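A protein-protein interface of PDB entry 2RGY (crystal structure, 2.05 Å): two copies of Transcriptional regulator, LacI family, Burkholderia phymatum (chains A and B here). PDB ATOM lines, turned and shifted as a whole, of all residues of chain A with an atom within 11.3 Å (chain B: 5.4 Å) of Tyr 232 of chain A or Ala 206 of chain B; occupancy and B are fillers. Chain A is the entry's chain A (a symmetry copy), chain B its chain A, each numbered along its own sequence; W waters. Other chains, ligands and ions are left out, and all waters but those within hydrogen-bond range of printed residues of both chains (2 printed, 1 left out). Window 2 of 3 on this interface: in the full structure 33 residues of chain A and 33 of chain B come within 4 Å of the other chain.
Printed residues of chain B within 4 Å of Tyr 232 of chain A: Pro 173, Glu 174, Tyr 177, Val 202, Ser 203 and Ala 206.
Printed residues of chain B within 4 Å of Ala 234 of chain A: Gln 209 (3.9 Å).
Printed residues of chain B within 4 Å of Pro 235 of chain A: Gln 209 (3.7 Å).
Pro 173 of chain B touches one residue of chain A.
Of chain A, only Tyr 232 (3.3 Å) comes within 4 Å of Glu 174 of chain B.
Of chain A, only Tyr 232 (3.8 Å) comes within 4 Å of Tyr 177 of chain B.
Of chain A, only Tyr 232 (3.8 Å) comes within 4 Å of Val 202 of chain B.
Of chain A, only Tyr 232 comes within 4 Å of Ser 203 of chain B.
No residue of chain A comes within 4 Å of Ala 204 of chain B.
No residue of chain A comes within 4 Å of Leu 205 of chain B.
Of chain A, only Tyr 232 (3.6 Å) comes within 4 Å of Ala 206 of chain B.
Of chain A, only Ala 234 and Pro 235 come within 4 Å of Gln 209 of chain B.
The nearest printed residue of chain B that does not touch Tyr 232 of chain A is Leu 205 of chain B (6.0 Å).
The nearest residue of chain A that does not touch Ala 206 of chain B is Ala 233 of chain A (4.2 Å).
The nearest printed residue of chain B that does not touch Ala 234 of chain A is Leu 205 of chain B (4.3 Å).
Of the 13 printed residues of chain B, 7 touch a printed residue of chain A.
Printed residues of chain B that touch a printed residue of chain A: Pro 173, Glu 174, Tyr 177, Val 202, Ser 203, Ala 206 and Gln 209.
Printed residues of chain A that touch a printed residue of chain B: Tyr 232, Ala 234 and Pro 235.
Along chain A the printed residues that touch a printed residue of chain B span positions 232 to 235.
Positions printed for both chains: 201, 202, 203, 205, 206 and 209.
Of the 8 pairs that touch across the chains among the printed residues, none has its exchanged pair printed and touching as well.
Water W2 bridges O of Val 215 of chain A (2.7 Å) and NE2 of Gln 209 of chain B (3.1 Å).
Water W1 lies within hydrogen-bond range of O of Tyr 232 of chain A, O of Val 202 of chain B and N of Ala 206 of chain B.
The backbone carbonyl oxygen (O) of Pro 173 of chain B lies within hydrogen-bond range of the side-chain hydroxyl (OG) of Ser 203 of chain B (2.6 Å).
OH of Tyr 177 of chain B sits at hydrogen-bond distance from OE1 of Gln 210 of chain B (2.6 Å).
CE1 of Tyr 232 of chain A touches CB of Pro 173 of chain B, at 3.7 Å.
CA of Glu 174 of chain B touches OH of Tyr 232 of chain A, at 3.3 Å.
CE2 of Tyr 232 of chain A touches CB of Tyr 177 of chain B, 3.8 Å away.
Val 202 of chain B touches Tyr 232 of chain A (CG1 to O, 3.8 Å).
Tyr 232 of chain A touches Ser 203 of chain B.
Tyr 232 of chain A touches Ala 206 of chain B.
Gln 209 of chain B touches Ala 234 of chain A.
Gln 209 of chain B touches Pro 235 of chain A (OE1 to CA, 3.7 Å).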
ATOM      1  N   SER A  21      28.615  -7.115   8.134  1.00  0.00           N
ATOM      2  CA  SER A  21      30.057  -7.257   8.311  1.00  0.00           C
ATOM      3  C   SER A  21      30.852  -6.278   7.438  1.00  0.00           C
ATOM      4  O   SER A  21      32.038  -6.043   7.661  1.00  0.00           O
ATOM      5  CB  SER A  21      30.486  -8.699   8.023  1.00  0.00           C
ATOM      6  OG  SER A  21      30.125  -9.095   6.712  1.00  0.00           O
ATOM      7  N   ASP A 198      25.690  -9.125  -0.332  1.00  0.00           N
ATOM      8  CA  ASP A 198      25.489 -10.409   0.334  1.00  0.00           C
ATOM      9  C   ASP A 198      24.272 -10.431   1.260  1.00  0.00           C
ATOM     10  O   ASP A 198      23.597 -11.456   1.370  1.00  0.00           O
ATOM     11  CB  ASP A 198      26.745 -10.804   1.126  1.00  0.00           C
ATOM     12  CG  ASP A 198      27.922 -11.163   0.222  1.00  0.00           C
ATOM     13  OD1 ASP A 198      27.715 -11.353  -0.995  1.00  0.00           O
ATOM     14  OD2 ASP A 198      29.057 -11.268   0.724  1.00  0.00           O
ATOM     15  N   ALA A 201      21.267 -11.033  -0.674  1.00  0.00           N
ATOM     16  CA  ALA A 201      21.422 -12.372  -1.241  1.00  0.00           C
ATOM     17  C   ALA A 201      21.027 -13.426  -0.215  1.00  0.00           C
ATOM     18  O   ALA A 201      20.365 -14.404  -0.542  1.00  0.00           O
ATOM     19  CB  ALA A 201      22.867 -12.600  -1.695  1.00  0.00           C
ATOM     20  N   VAL A 202      21.446 -13.230   1.027  1.00  0.00           N
ATOM     21  CA  VAL A 202      21.116 -14.179   2.079  1.00  0.00           C
ATOM     22  C   VAL A 202      19.610 -14.240   2.276  1.00  0.00           C
ATOM     23  O   VAL A 202      19.063 -15.320   2.471  1.00  0.00           O
ATOM     24  CB  VAL A 202      21.796 -13.805   3.400  1.00  0.00           C
ATOM     25  CG1 VAL A 202      21.243 -14.667   4.535  1.00  0.00           C
ATOM     26  CG2 VAL A 202      23.291 -14.006   3.266  1.00  0.00           C
ATOM     27  N   SER A 203      18.942 -13.091   2.223  1.00  0.00           N
ATOM     28  CA  SER A 203      17.485 -13.065   2.360  1.00  0.00           C
ATOM     29  C   SER A 203      16.838 -13.816   1.188  1.00  0.00           C
ATOM     30  O   SER A 203      15.795 -14.439   1.343  1.00  0.00           O
ATOM     31  CB  SER A 203      16.959 -11.621   2.391  1.00  0.00           C
ATOM     32  OG  SER A 203      17.292 -10.972   3.610  1.00  0.00           O
ATOM     33  N   LEU A 205      18.103 -16.389  -0.324  1.00  0.00           N
ATOM     34  CA  LEU A 205      18.303 -17.789  -0.002  1.00  0.00           C
ATOM     35  C   LEU A 205      17.274 -18.203   1.038  1.00  0.00           C
ATOM     36  O   LEU A 205      16.866 -19.364   1.089  1.00  0.00           O
ATOM     37  CB  LEU A 205      19.708 -18.018   0.562  1.00  0.00           C
ATOM     38  CG  LEU A 205      20.878 -17.788  -0.403  1.00  0.00           C
ATOM     39  CD1 LEU A 205      22.191 -18.125   0.298  1.00  0.00           C
ATOM     40  CD2 LEU A 205      20.700 -18.649  -1.632  1.00  0.00           C
ATOM     41  N   ALA A 206      16.864 -17.243   1.868  1.00  0.00           N
ATOM     42  CA  ALA A 206      15.890 -17.506   2.920  1.00  0.00           C
ATOM     43  C   ALA A 206      14.537 -17.808   2.314  1.00  0.00           C
ATOM     44  O   ALA A 206      13.884 -18.766   2.707  1.00  0.00           O
ATOM     45  CB  ALA A 206      15.782 -16.317   3.859  1.00  0.00           C
ATOM     46  N   GLN A 209      14.408 -21.107   0.278  1.00  0.00           N
ATOM     47  CA  GLN A 209      14.351 -22.267   1.159  1.00  0.00           C
ATOM     48  C   GLN A 209      12.924 -22.465   1.677  1.00  0.00           C
ATOM     49  O   GLN A 209      12.451 -23.598   1.794  1.00  0.00           O
ATOM     50  CB  GLN A 209      15.334 -22.094   2.324  1.00  0.00           C
ATOM     51  CG  GLN A 209      15.634 -23.361   3.144  1.00  0.00           C
ATOM     52  CD  GLN A 209      14.535 -23.718   4.135  1.00  0.00           C
ATOM     53  OE1 GLN A 209      13.803 -22.847   4.606  1.00  0.00           O
ATOM     54  NE2 GLN A 209      14.431 -25.003   4.473  1.00  0.00           N
ATOM     55  N   VAL A 215      18.914 -24.185  -4.261  1.00  0.00           N
ATOM     56  CA  VAL A 215      20.040 -23.372  -4.671  1.00  0.00           C
ATOM     57  C   VAL A 215      21.268 -24.220  -4.382  1.00  0.00           C
ATOM     58  O   VAL A 215      21.467 -24.654  -3.252  1.00  0.00           O
ATOM     59  CB  VAL A 215      20.103 -22.067  -3.850  1.00  0.00           C
ATOM     60  CG1 VAL A 215      21.330 -21.257  -4.245  1.00  0.00           C
ATOM     61  CG2 VAL A 215      18.841 -21.267  -4.071  1.00  0.00           C
ATOM     62  N   ASP A 226      31.352 -10.093  -0.456  1.00  0.00           N
ATOM     63  CA  ASP A 226      32.031 -11.277   0.076  1.00  0.00           C
ATOM     64  C   ASP A 226      32.237 -11.007   1.554  1.00  0.00           C
ATOM     65  O   ASP A 226      33.331 -11.175   2.110  1.00  0.00           O
ATOM     66  CB  ASP A 226      33.373 -11.557  -0.612  1.00  0.00           C
ATOM     67  CG  ASP A 226      33.969 -12.902  -0.192  1.00  0.00           C
ATOM     68  OD1 ASP A 226      33.202 -13.764   0.293  1.00  0.00           O
ATOM     69  OD2 ASP A 226      35.192 -13.105  -0.356  1.00  0.00           O
ATOM     70  N   ASP A 227      31.152 -10.552   2.174  1.00  0.00           N
ATOM     71  CA  ASP A 227      31.139 -10.248   3.589  1.00  0.00           C
ATOM     72  C   ASP A 227      31.322 -11.597   4.275  1.00  0.00           C
ATOM     73  O   ASP A 227      30.985 -12.640   3.703  1.00  0.00           O
ATOM     74  CB  ASP A 227      29.812  -9.552   3.930  1.00  0.00           C
ATOM     75  CG  ASP A 227      29.866  -8.040   3.654  1.00  0.00           C
ATOM     76  OD1 ASP A 227      28.805  -7.424   3.397  1.00  0.00           O
ATOM     77  OD2 ASP A 227      30.981  -7.459   3.712  1.00  0.00           O
ATOM     78  N   TYR A 228      31.868 -11.616   5.480  1.00  0.00           N
ATOM     79  CA  TYR A 228      32.094 -12.918   6.070  1.00  0.00           C
ATOM     80  C   TYR A 228      30.921 -13.663   6.681  1.00  0.00           C
ATOM     81  O   TYR A 228      31.084 -14.554   7.508  1.00  0.00           O
ATOM     82  CB  TYR A 228      33.321 -12.853   6.980  1.00  0.00           C
ATOM     83  CG  TYR A 228      34.583 -12.755   6.134  1.00  0.00           C
ATOM     84  CD1 TYR A 228      35.723 -12.085   6.596  1.00  0.00           C
ATOM     85  CD2 TYR A 228      34.635 -13.350   4.856  1.00  0.00           C
ATOM     86  CE1 TYR A 228      36.890 -12.008   5.806  1.00  0.00           C
ATOM     87  CE2 TYR A 228      35.795 -13.280   4.066  1.00  0.00           C
ATOM     88  CZ  TYR A 228      36.915 -12.610   4.548  1.00  0.00           C
ATOM     89  OH  TYR A 228      38.067 -12.571   3.775  1.00  0.00           O
ATOM     90  N   SER A 229      29.730 -13.316   6.213  1.00  0.00           N
ATOM     91  CA  SER A 229      28.517 -14.004   6.627  1.00  0.00           C
ATOM     92  C   SER A 229      28.197 -14.959   5.466  1.00  0.00           C
ATOM     93  O   SER A 229      27.359 -15.861   5.593  1.00  0.00           O
ATOM     94  CB  SER A 229      27.368 -13.005   6.807  1.00  0.00           C
ATOM     95  OG  SER A 229      26.139 -13.675   7.080  1.00  0.00           O
ATOM     96  N   ALA A 230      28.887 -14.759   4.341  1.00  0.00           N
ATOM     97  CA  ALA A 230      28.676 -15.561   3.133  1.00  0.00           C
ATOM     98  C   ALA A 230      29.145 -17.006   3.218  1.00  0.00           C
ATOM     99  O   ALA A 230      28.428 -17.921   2.801  1.00  0.00           O
ATOM    100  CB  ALA A 230      29.334 -14.872   1.931  1.00  0.00           C
ATOM    101  N   ALA A 231      30.345 -17.218   3.752  1.00  0.00           N
ATOM    102  CA  ALA A 231      30.884 -18.569   3.864  1.00  0.00           C
ATOM    103  C   ALA A 231      29.978 -19.465   4.690  1.00  0.00           C
ATOM    104  O   ALA A 231      29.978 -20.682   4.522  1.00  0.00           O
ATOM    105  CB  ALA A 231      32.282 -18.536   4.486  1.00  0.00           C
ATOM    106  N   TYR A 232      29.193 -18.862   5.573  1.00  0.00           N
ATOM    107  CA  TYR A 232      28.308 -19.635   6.430  1.00  0.00           C
ATOM    108  C   TYR A 232      26.837 -19.552   6.063  1.00  0.00           C
ATOM    109  O   TYR A 232      25.966 -19.861   6.878  1.00  0.00           O
ATOM    110  CB  TYR A 232      28.522 -19.223   7.880  1.00  0.00           C
ATOM    111  CG  TYR A 232      29.961 -19.391   8.271  1.00  0.00           C
ATOM    112  CD1 TYR A 232      30.831 -18.300   8.303  1.00  0.00           C
ATOM    113  CD2 TYR A 232      30.474 -20.658   8.548  1.00  0.00           C
ATOM    114  CE1 TYR A 232      32.182 -18.471   8.605  1.00  0.00           C
ATOM    115  CE2 TYR A 232      31.814 -20.836   8.844  1.00  0.00           C
ATOM    116  CZ  TYR A 232      32.660 -19.743   8.876  1.00  0.00           C
ATOM    117  OH  TYR A 232      33.976 -19.936   9.214  1.00  0.00           O
ATOM    118  N   ALA A 233      26.564 -19.131   4.835  1.00  0.00           N
ATOM    119  CA  ALA A 233      25.199 -19.062   4.357  1.00  0.00           C
ATOM    120  C   ALA A 233      24.837 -20.498   3.997  1.00  0.00           C
ATOM    121  O   ALA A 233      25.715 -21.360   3.885  1.00  0.00           O
ATOM    122  CB  ALA A 233      25.109 -18.171   3.119  1.00  0.00           C
ATOM    123  N   ALA A 234      23.550 -20.763   3.826  1.00  0.00           N
ATOM    124  CA  ALA A 234      23.114 -22.105   3.467  1.00  0.00           C
ATOM    125  C   ALA A 234      22.329 -22.029   2.170  1.00  0.00           C
ATOM    126  O   ALA A 234      21.166 -21.625   2.164  1.00  0.00           O
ATOM    127  CB  ALA A 234      22.241 -22.691   4.568  1.00  0.00           C
ATOM    128  N   PRO A 235      22.950 -22.428   1.050  1.00  0.00           N
ATOM    129  CA  PRO A 235      24.320 -22.945   0.907  1.00  0.00           C
ATOM    130  C   PRO A 235      25.377 -21.842   0.947  1.00  0.00           C
ATOM    131  O   PRO A 235      25.043 -20.658   0.881  1.00  0.00           O
ATOM    132  CB  PRO A 235      24.271 -23.628  -0.449  1.00  0.00           C
ATOM    133  CG  PRO A 235      23.379 -22.694  -1.226  1.00  0.00           C
ATOM    134  CD  PRO A 235      22.246 -22.470  -0.244  1.00  0.00           C
ATOM    135  N   ALA A 236      26.646 -22.233   1.044  1.00  0.00           N
ATOM    136  CA  ALA A 236      27.741 -21.265   1.084  1.00  0.00           C
ATOM    137  C   ALA A 236      27.589 -20.328  -0.114  1.00  0.00           C
ATOM    138  O   ALA A 236      27.534 -20.778  -1.256  1.00  0.00           O
ATOM    139  CB  ALA A 236      29.082 -21.982   1.038  1.00  0.00           C
ATOM    140  N   LEU A 237      27.524 -19.027   0.161  1.00  0.00           N
ATOM    141  CA  LEU A 237      27.300 -18.024  -0.879  1.00  0.00           C
ATOM    142  C   LEU A 237      28.489 -17.607  -1.733  1.00  0.00           C
ATOM    143  O   LEU A 237      29.499 -17.113  -1.215  1.00  0.00           O
ATOM    144  CB  LEU A 237      26.689 -16.766  -0.256  1.00  0.00           C
ATOM    145  CG  LEU A 237      26.306 -15.639  -1.216  1.00  0.00           C
ATOM    146  CD1 LEU A 237      25.130 -16.082  -2.086  1.00  0.00           C
ATOM    147  CD2 LEU A 237      25.948 -14.393  -0.420  1.00  0.00           C
ATOM    148  N   THR A 238      28.350 -17.802  -3.045  1.00  0.00           N
ATOM    149  CA  THR A 238      29.377 -17.401  -4.002  1.00  0.00           C
ATOM    150  C   THR A 238      29.194 -15.894  -4.101  1.00  0.00           C
ATOM    151  O   THR A 238      28.081 -15.403  -4.293  1.00  0.00           O
ATOM    152  CB  THR A 238      29.157 -18.073  -5.377  1.00  0.00           C
ATOM    153  OG1 THR A 238      29.442 -19.478  -5.264  1.00  0.00           O
ATOM    154  CG2 THR A 238      30.068 -17.450  -6.437  1.00  0.00           C
ATOM    155  N   SER A 239      30.285 -15.154  -3.957  1.00  0.00           N
ATOM    156  CA  SER A 239      30.193 -13.706  -3.961  1.00  0.00           C
ATOM    157  C   SER A 239      31.380 -13.005  -4.601  1.00  0.00           C
ATOM    158  O   SER A 239      32.487 -13.528  -4.612  1.00  0.00           O
ATOM    159  CB  SER A 239      30.040 -13.225  -2.510  1.00  0.00           C
ATOM    160  OG  SER A 239      29.923 -11.815  -2.410  1.00  0.00           O
ATOM    161  N   SER A 275      34.643 -15.072  -5.185  1.00  0.00           N
ATOM    162  CA  SER A 275      34.838 -16.126  -4.210  1.00  0.00           C
ATOM    163  C   SER A 275      33.828 -17.220  -4.520  1.00  0.00           C
ATOM    164  O   SER A 275      32.663 -17.128  -4.148  1.00  0.00           O
ATOM    165  CB  SER A 275      34.636 -15.577  -2.799  1.00  0.00           C
ATOM    166  OG  SER A 275      35.574 -14.546  -2.550  1.00  0.00           O
ATOM    167  N   MET A 276      34.283 -18.243  -5.232  1.00  0.00           N
ATOM    168  CA  MET A 276      33.418 -19.347  -5.619  1.00  0.00           C
ATOM    169  C   MET A 276      33.117 -20.263  -4.449  1.00  0.00           C
ATOM    170  O   MET A 276      34.026 -20.828  -3.842  1.00  0.00           O
ATOM    171  CB  MET A 276      34.063 -20.172  -6.742  1.00  0.00           C
ATOM    172  CG  MET A 276      33.989 -19.563  -8.138  1.00  0.00           C
ATOM    173  SD  MET A 276      32.308 -19.410  -8.832  1.00  0.00           S
ATOM    174  CE  MET A 276      31.625 -21.003  -8.488  1.00  0.00           C
ATOM    175  N   ARG A 277      31.836 -20.405  -4.133  1.00  0.00           N
ATOM    176  CA  ARG A 277      31.440 -21.280  -3.039  1.00  0.00           C
ATOM    177  C   ARG A 277      30.443 -22.294  -3.564  1.00  0.00           C
ATOM    178  O   ARG A 277      30.725 -22.944  -4.569  1.00  0.00           O
ATOM    179  CB  ARG A 277      30.890 -20.453  -1.870  1.00  0.00           C
ATOM    180  CG  ARG A 277      31.944 -19.475  -1.332  1.00  0.00           C
ATOM    181  CD  ARG A 277      31.789 -19.201   0.153  1.00  0.00           C
ATOM    182  NE  ARG A 277      32.857 -18.353   0.685  1.00  0.00           N
ATOM    183  CZ  ARG A 277      32.962 -17.046   0.467  1.00  0.00           C
ATOM    184  NH1 ARG A 277      32.060 -16.419  -0.278  1.00  0.00           N
ATOM    185  NH2 ARG A 277      33.962 -16.362   1.004  1.00  0.00           N
ATOM    186  N   ALA A 278      29.271 -22.417  -2.948  1.00  0.00           N
ATOM    187  CA  ALA A 278      28.327 -23.424  -3.414  1.00  0.00           C
ATOM    188  C   ALA A 278      26.964 -22.962  -3.908  1.00  0.00           C
ATOM    189  O   ALA A 278      26.095 -23.795  -4.173  1.00  0.00           O
ATOM    190  CB  ALA A 278      28.142 -24.476  -2.322  1.00  0.00           C
ATOM    191  N   SER A 279      26.758 -21.659  -4.050  1.00  0.00           N
ATOM    192  CA  SER A 279      25.454 -21.171  -4.486  1.00  0.00           C
ATOM    193  C   SER A 279      25.303 -21.033  -5.997  1.00  0.00           C
ATOM    194  O   SER A 279      24.221 -20.730  -6.482  1.00  0.00           O
ATOM    195  CB  SER A 279      25.140 -19.830  -3.826  1.00  0.00           C
ATOM    196  OG  SER A 279      26.100 -18.878  -4.208  1.00  0.00           O
ATOM    197  N   PRO B 173      31.564 -17.406  14.179  1.00  0.00           N
ATOM    198  CA  PRO B 173      31.032 -18.198  13.066  1.00  0.00           C
ATOM    199  C   PRO B 173      31.845 -19.469  12.831  1.00  0.00           C
ATOM    200  O   PRO B 173      31.282 -20.560  12.735  1.00  0.00           O
ATOM    201  CB  PRO B 173      31.124 -17.238  11.877  1.00  0.00           C
ATOM    202  CG  PRO B 173      30.961 -15.899  12.512  1.00  0.00           C
ATOM    203  CD  PRO B 173      31.829 -16.023  13.746  1.00  0.00           C
ATOM    204  N   GLU B 174      33.164 -19.319  12.734  1.00  0.00           N
ATOM    205  CA  GLU B 174      34.055 -20.458  12.502  1.00  0.00           C
ATOM    206  C   GLU B 174      34.042 -21.438  13.677  1.00  0.00           C
ATOM    207  O   GLU B 174      34.163 -22.649  13.483  1.00  0.00           O
ATOM    208  CB  GLU B 174      35.489 -19.980  12.259  1.00  0.00           C
ATOM    209  CG  GLU B 174      36.092 -19.234  13.444  1.00  0.00           C
ATOM    210  CD  GLU B 174      35.867 -17.728  13.382  1.00  0.00           C
ATOM    211  OE1 GLU B 174      34.810 -17.293  12.872  1.00  0.00           O
ATOM    212  OE2 GLU B 174      36.754 -16.979  13.859  1.00  0.00           O
ATOM    213  N   TYR B 177      30.933 -23.573  13.442  1.00  0.00           N
ATOM    214  CA  TYR B 177      31.040 -24.529  12.349  1.00  0.00           C
ATOM    215  C   TYR B 177      31.875 -25.729  12.770  1.00  0.00           C
ATOM    216  O   TYR B 177      31.488 -26.881  12.558  1.00  0.00           O
ATOM    217  CB  TYR B 177      31.681 -23.880  11.121  1.00  0.00           C
ATOM    218  CG  TYR B 177      31.717 -24.787   9.914  1.00  0.00           C
ATOM    219  CD1 TYR B 177      30.564 -25.035   9.171  1.00  0.00           C
ATOM    220  CD2 TYR B 177      32.910 -25.399   9.510  1.00  0.00           C
ATOM    221  CE1 TYR B 177      30.596 -25.868   8.052  1.00  0.00           C
ATOM    222  CE2 TYR B 177      32.951 -26.237   8.396  1.00  0.00           C
ATOM    223  CZ  TYR B 177      31.790 -26.468   7.671  1.00  0.00           C
ATOM    224  OH  TYR B 177      31.811 -27.313   6.575  1.00  0.00           O
ATOM    225  N   ALA B 201      24.723 -20.949  15.881  1.00  0.00           N
ATOM    226  CA  ALA B 201      23.555 -21.694  15.412  1.00  0.00           C
ATOM    227  C   ALA B 201      23.468 -21.631  13.892  1.00  0.00           C
ATOM    228  O   ALA B 201      23.171 -22.625  13.238  1.00  0.00           O
ATOM    229  CB  ALA B 201      22.272 -21.131  16.033  1.00  0.00           C
ATOM    230  N   VAL B 202      23.715 -20.456  13.332  1.00  0.00           N
ATOM    231  CA  VAL B 202      23.662 -20.296  11.888  1.00  0.00           C
ATOM    232  C   VAL B 202      24.712 -21.172  11.225  1.00  0.00           C
ATOM    233  O   VAL B 202      24.442 -21.775  10.192  1.00  0.00           O
ATOM    234  CB  VAL B 202      23.874 -18.835  11.480  1.00  0.00           C
ATOM    235  CG1 VAL B 202      24.056 -18.736   9.965  1.00  0.00           C
ATOM    236  CG2 VAL B 202      22.680 -18.015  11.921  1.00  0.00           C
ATOM    237  N   SER B 203      25.903 -21.245  11.813  1.00  0.00           N
ATOM    238  CA  SER B 203      26.958 -22.099  11.264  1.00  0.00           C
ATOM    239  C   SER B 203      26.525 -23.570  11.331  1.00  0.00           C
ATOM    240  O   SER B 203      26.878 -24.367  10.469  1.00  0.00           O
ATOM    241  CB  SER B 203      28.273 -21.921  12.040  1.00  0.00           C
ATOM    242  OG  SER B 203      28.868 -20.659  11.772  1.00  0.00           O
ATOM    243  N   ALA B 204      25.760 -23.927  12.362  1.00  0.00           N
ATOM    244  CA  ALA B 204      25.288 -25.302  12.499  1.00  0.00           C
ATOM    245  C   ALA B 204      24.337 -25.617  11.348  1.00  0.00           C
ATOM    246  O   ALA B 204      24.378 -26.708  10.767  1.00  0.00           O
ATOM    247  CB  ALA B 204      24.582 -25.491  13.830  1.00  0.00           C
ATOM    248  N   LEU B 205      23.484 -24.651  11.025  1.00  0.00           N
ATOM    249  CA  LEU B 205      22.535 -24.791   9.936  1.00  0.00           C
ATOM    250  C   LEU B 205      23.305 -24.911   8.631  1.00  0.00           C
ATOM    251  O   LEU B 205      22.839 -25.548   7.685  1.00  0.00           O
ATOM    252  CB  LEU B 205      21.612 -23.572   9.865  1.00  0.00           C
ATOM    253  CG  LEU B 205      20.651 -23.373  11.044  1.00  0.00           C
ATOM    254  CD1 LEU B 205      19.763 -22.159  10.779  1.00  0.00           C
ATOM    255  CD2 LEU B 205      19.807 -24.613  11.227  1.00  0.00           C
ATOM    256  N   ALA B 206      24.483 -24.290   8.588  1.00  0.00           N
ATOM    257  CA  ALA B 206      25.317 -24.314   7.393  1.00  0.00           C
ATOM    258  C   ALA B 206      25.844 -25.711   7.153  1.00  0.00           C
ATOM    259  O   ALA B 206      25.790 -26.209   6.036  1.00  0.00           O
ATOM    260  CB  ALA B 206      26.477 -23.341   7.529  1.00  0.00           C
ATOM    261  N   ARG B 207      26.353 -26.339   8.209  1.00  0.00           N
ATOM    262  CA  ARG B 207      26.900 -27.687   8.125  1.00  0.00           C
ATOM    263  C   ARG B 207      25.809 -28.693   7.795  1.00  0.00           C
ATOM    264  O   ARG B 207      25.961 -29.499   6.888  1.00  0.00           O
ATOM    265  CB  ARG B 207      27.579 -28.069   9.448  1.00  0.00           C
ATOM    266  CG  ARG B 207      28.283 -29.420   9.419  1.00  0.00           C
ATOM    267  CD  ARG B 207      29.138 -29.551   8.166  1.00  0.00           C
ATOM    268  NE  ARG B 207      29.924 -30.778   8.153  1.00  0.00           N
ATOM    269  CZ  ARG B 207      30.570 -31.244   7.085  1.00  0.00           C
ATOM    270  NH1 ARG B 207      30.523 -30.588   5.935  1.00  0.00           N
ATOM    271  NH2 ARG B 207      31.257 -32.375   7.166  1.00  0.00           N
ATOM    272  N   PHE B 208      24.706 -28.638   8.533  1.00  0.00           N
ATOM    273  CA  PHE B 208      23.594 -29.549   8.295  1.00  0.00           C
ATOM    274  C   PHE B 208      23.134 -29.503   6.841  1.00  0.00           C
ATOM    275  O   PHE B 208      22.800 -30.531   6.264  1.00  0.00           O
ATOM    276  CB  PHE B 208      22.415 -29.198   9.205  1.00  0.00           C
ATOM    277  CG  PHE B 208      22.666 -29.481  10.661  1.00  0.00           C
ATOM    278  CD1 PHE B 208      21.788 -28.998  11.633  1.00  0.00           C
ATOM    279  CD2 PHE B 208      23.778 -30.230  11.066  1.00  0.00           C
ATOM    280  CE1 PHE B 208      22.000 -29.252  12.987  1.00  0.00           C
ATOM    281  CE2 PHE B 208      24.006 -30.496  12.430  1.00  0.00           C
ATOM    282  CZ  PHE B 208      23.107 -29.998  13.392  1.00  0.00           C
ATOM    283  N   GLN B 209      23.108 -28.309   6.255  1.00  0.00           N
ATOM    284  CA  GLN B 209      22.674 -28.160   4.872  1.00  0.00           C
ATOM    285  C   GLN B 209      23.685 -28.816   3.929  1.00  0.00           C
ATOM    286  O   GLN B 209      23.304 -29.441   2.937  1.00  0.00           O
ATOM    287  CB  GLN B 209      22.497 -26.673   4.532  1.00  0.00           C
ATOM    288  CG  GLN B 209      21.730 -26.368   3.233  1.00  0.00           C
ATOM    289  CD  GLN B 209      22.568 -26.548   1.975  1.00  0.00           C
ATOM    290  OE1 GLN B 209      23.791 -26.408   2.008  1.00  0.00           O
ATOM    291  NE2 GLN B 209      21.907 -26.836   0.854  1.00  0.00           N
ATOM    292  N   GLN B 210      24.968 -28.693   4.254  1.00  0.00           N
ATOM    293  CA  GLN B 210      26.018 -29.292   3.435  1.00  0.00           C
ATOM    294  C   GLN B 210      25.930 -30.823   3.429  1.00  0.00           C
ATOM    295  O   GLN B 210      26.306 -31.459   2.446  1.00  0.00           O
ATOM    296  CB  GLN B 210      27.409 -28.875   3.942  1.00  0.00           C
ATOM    297  CG  GLN B 210      27.673 -27.374   3.902  1.00  0.00           C
ATOM    298  CD  GLN B 210      29.035 -26.990   4.465  1.00  0.00           C
ATOM    299  OE1 GLN B 210      29.736 -27.807   5.065  1.00  0.00           O
ATOM    300  NE2 GLN B 210      29.406 -25.726   4.291  1.00  0.00           N
HETATM  301  O   HOH W   1      23.541 -21.085   7.571  1.00  0.00           O
HETATM  302  O   HOH W   2      22.736 -26.739  -2.114  1.00  0.00           O
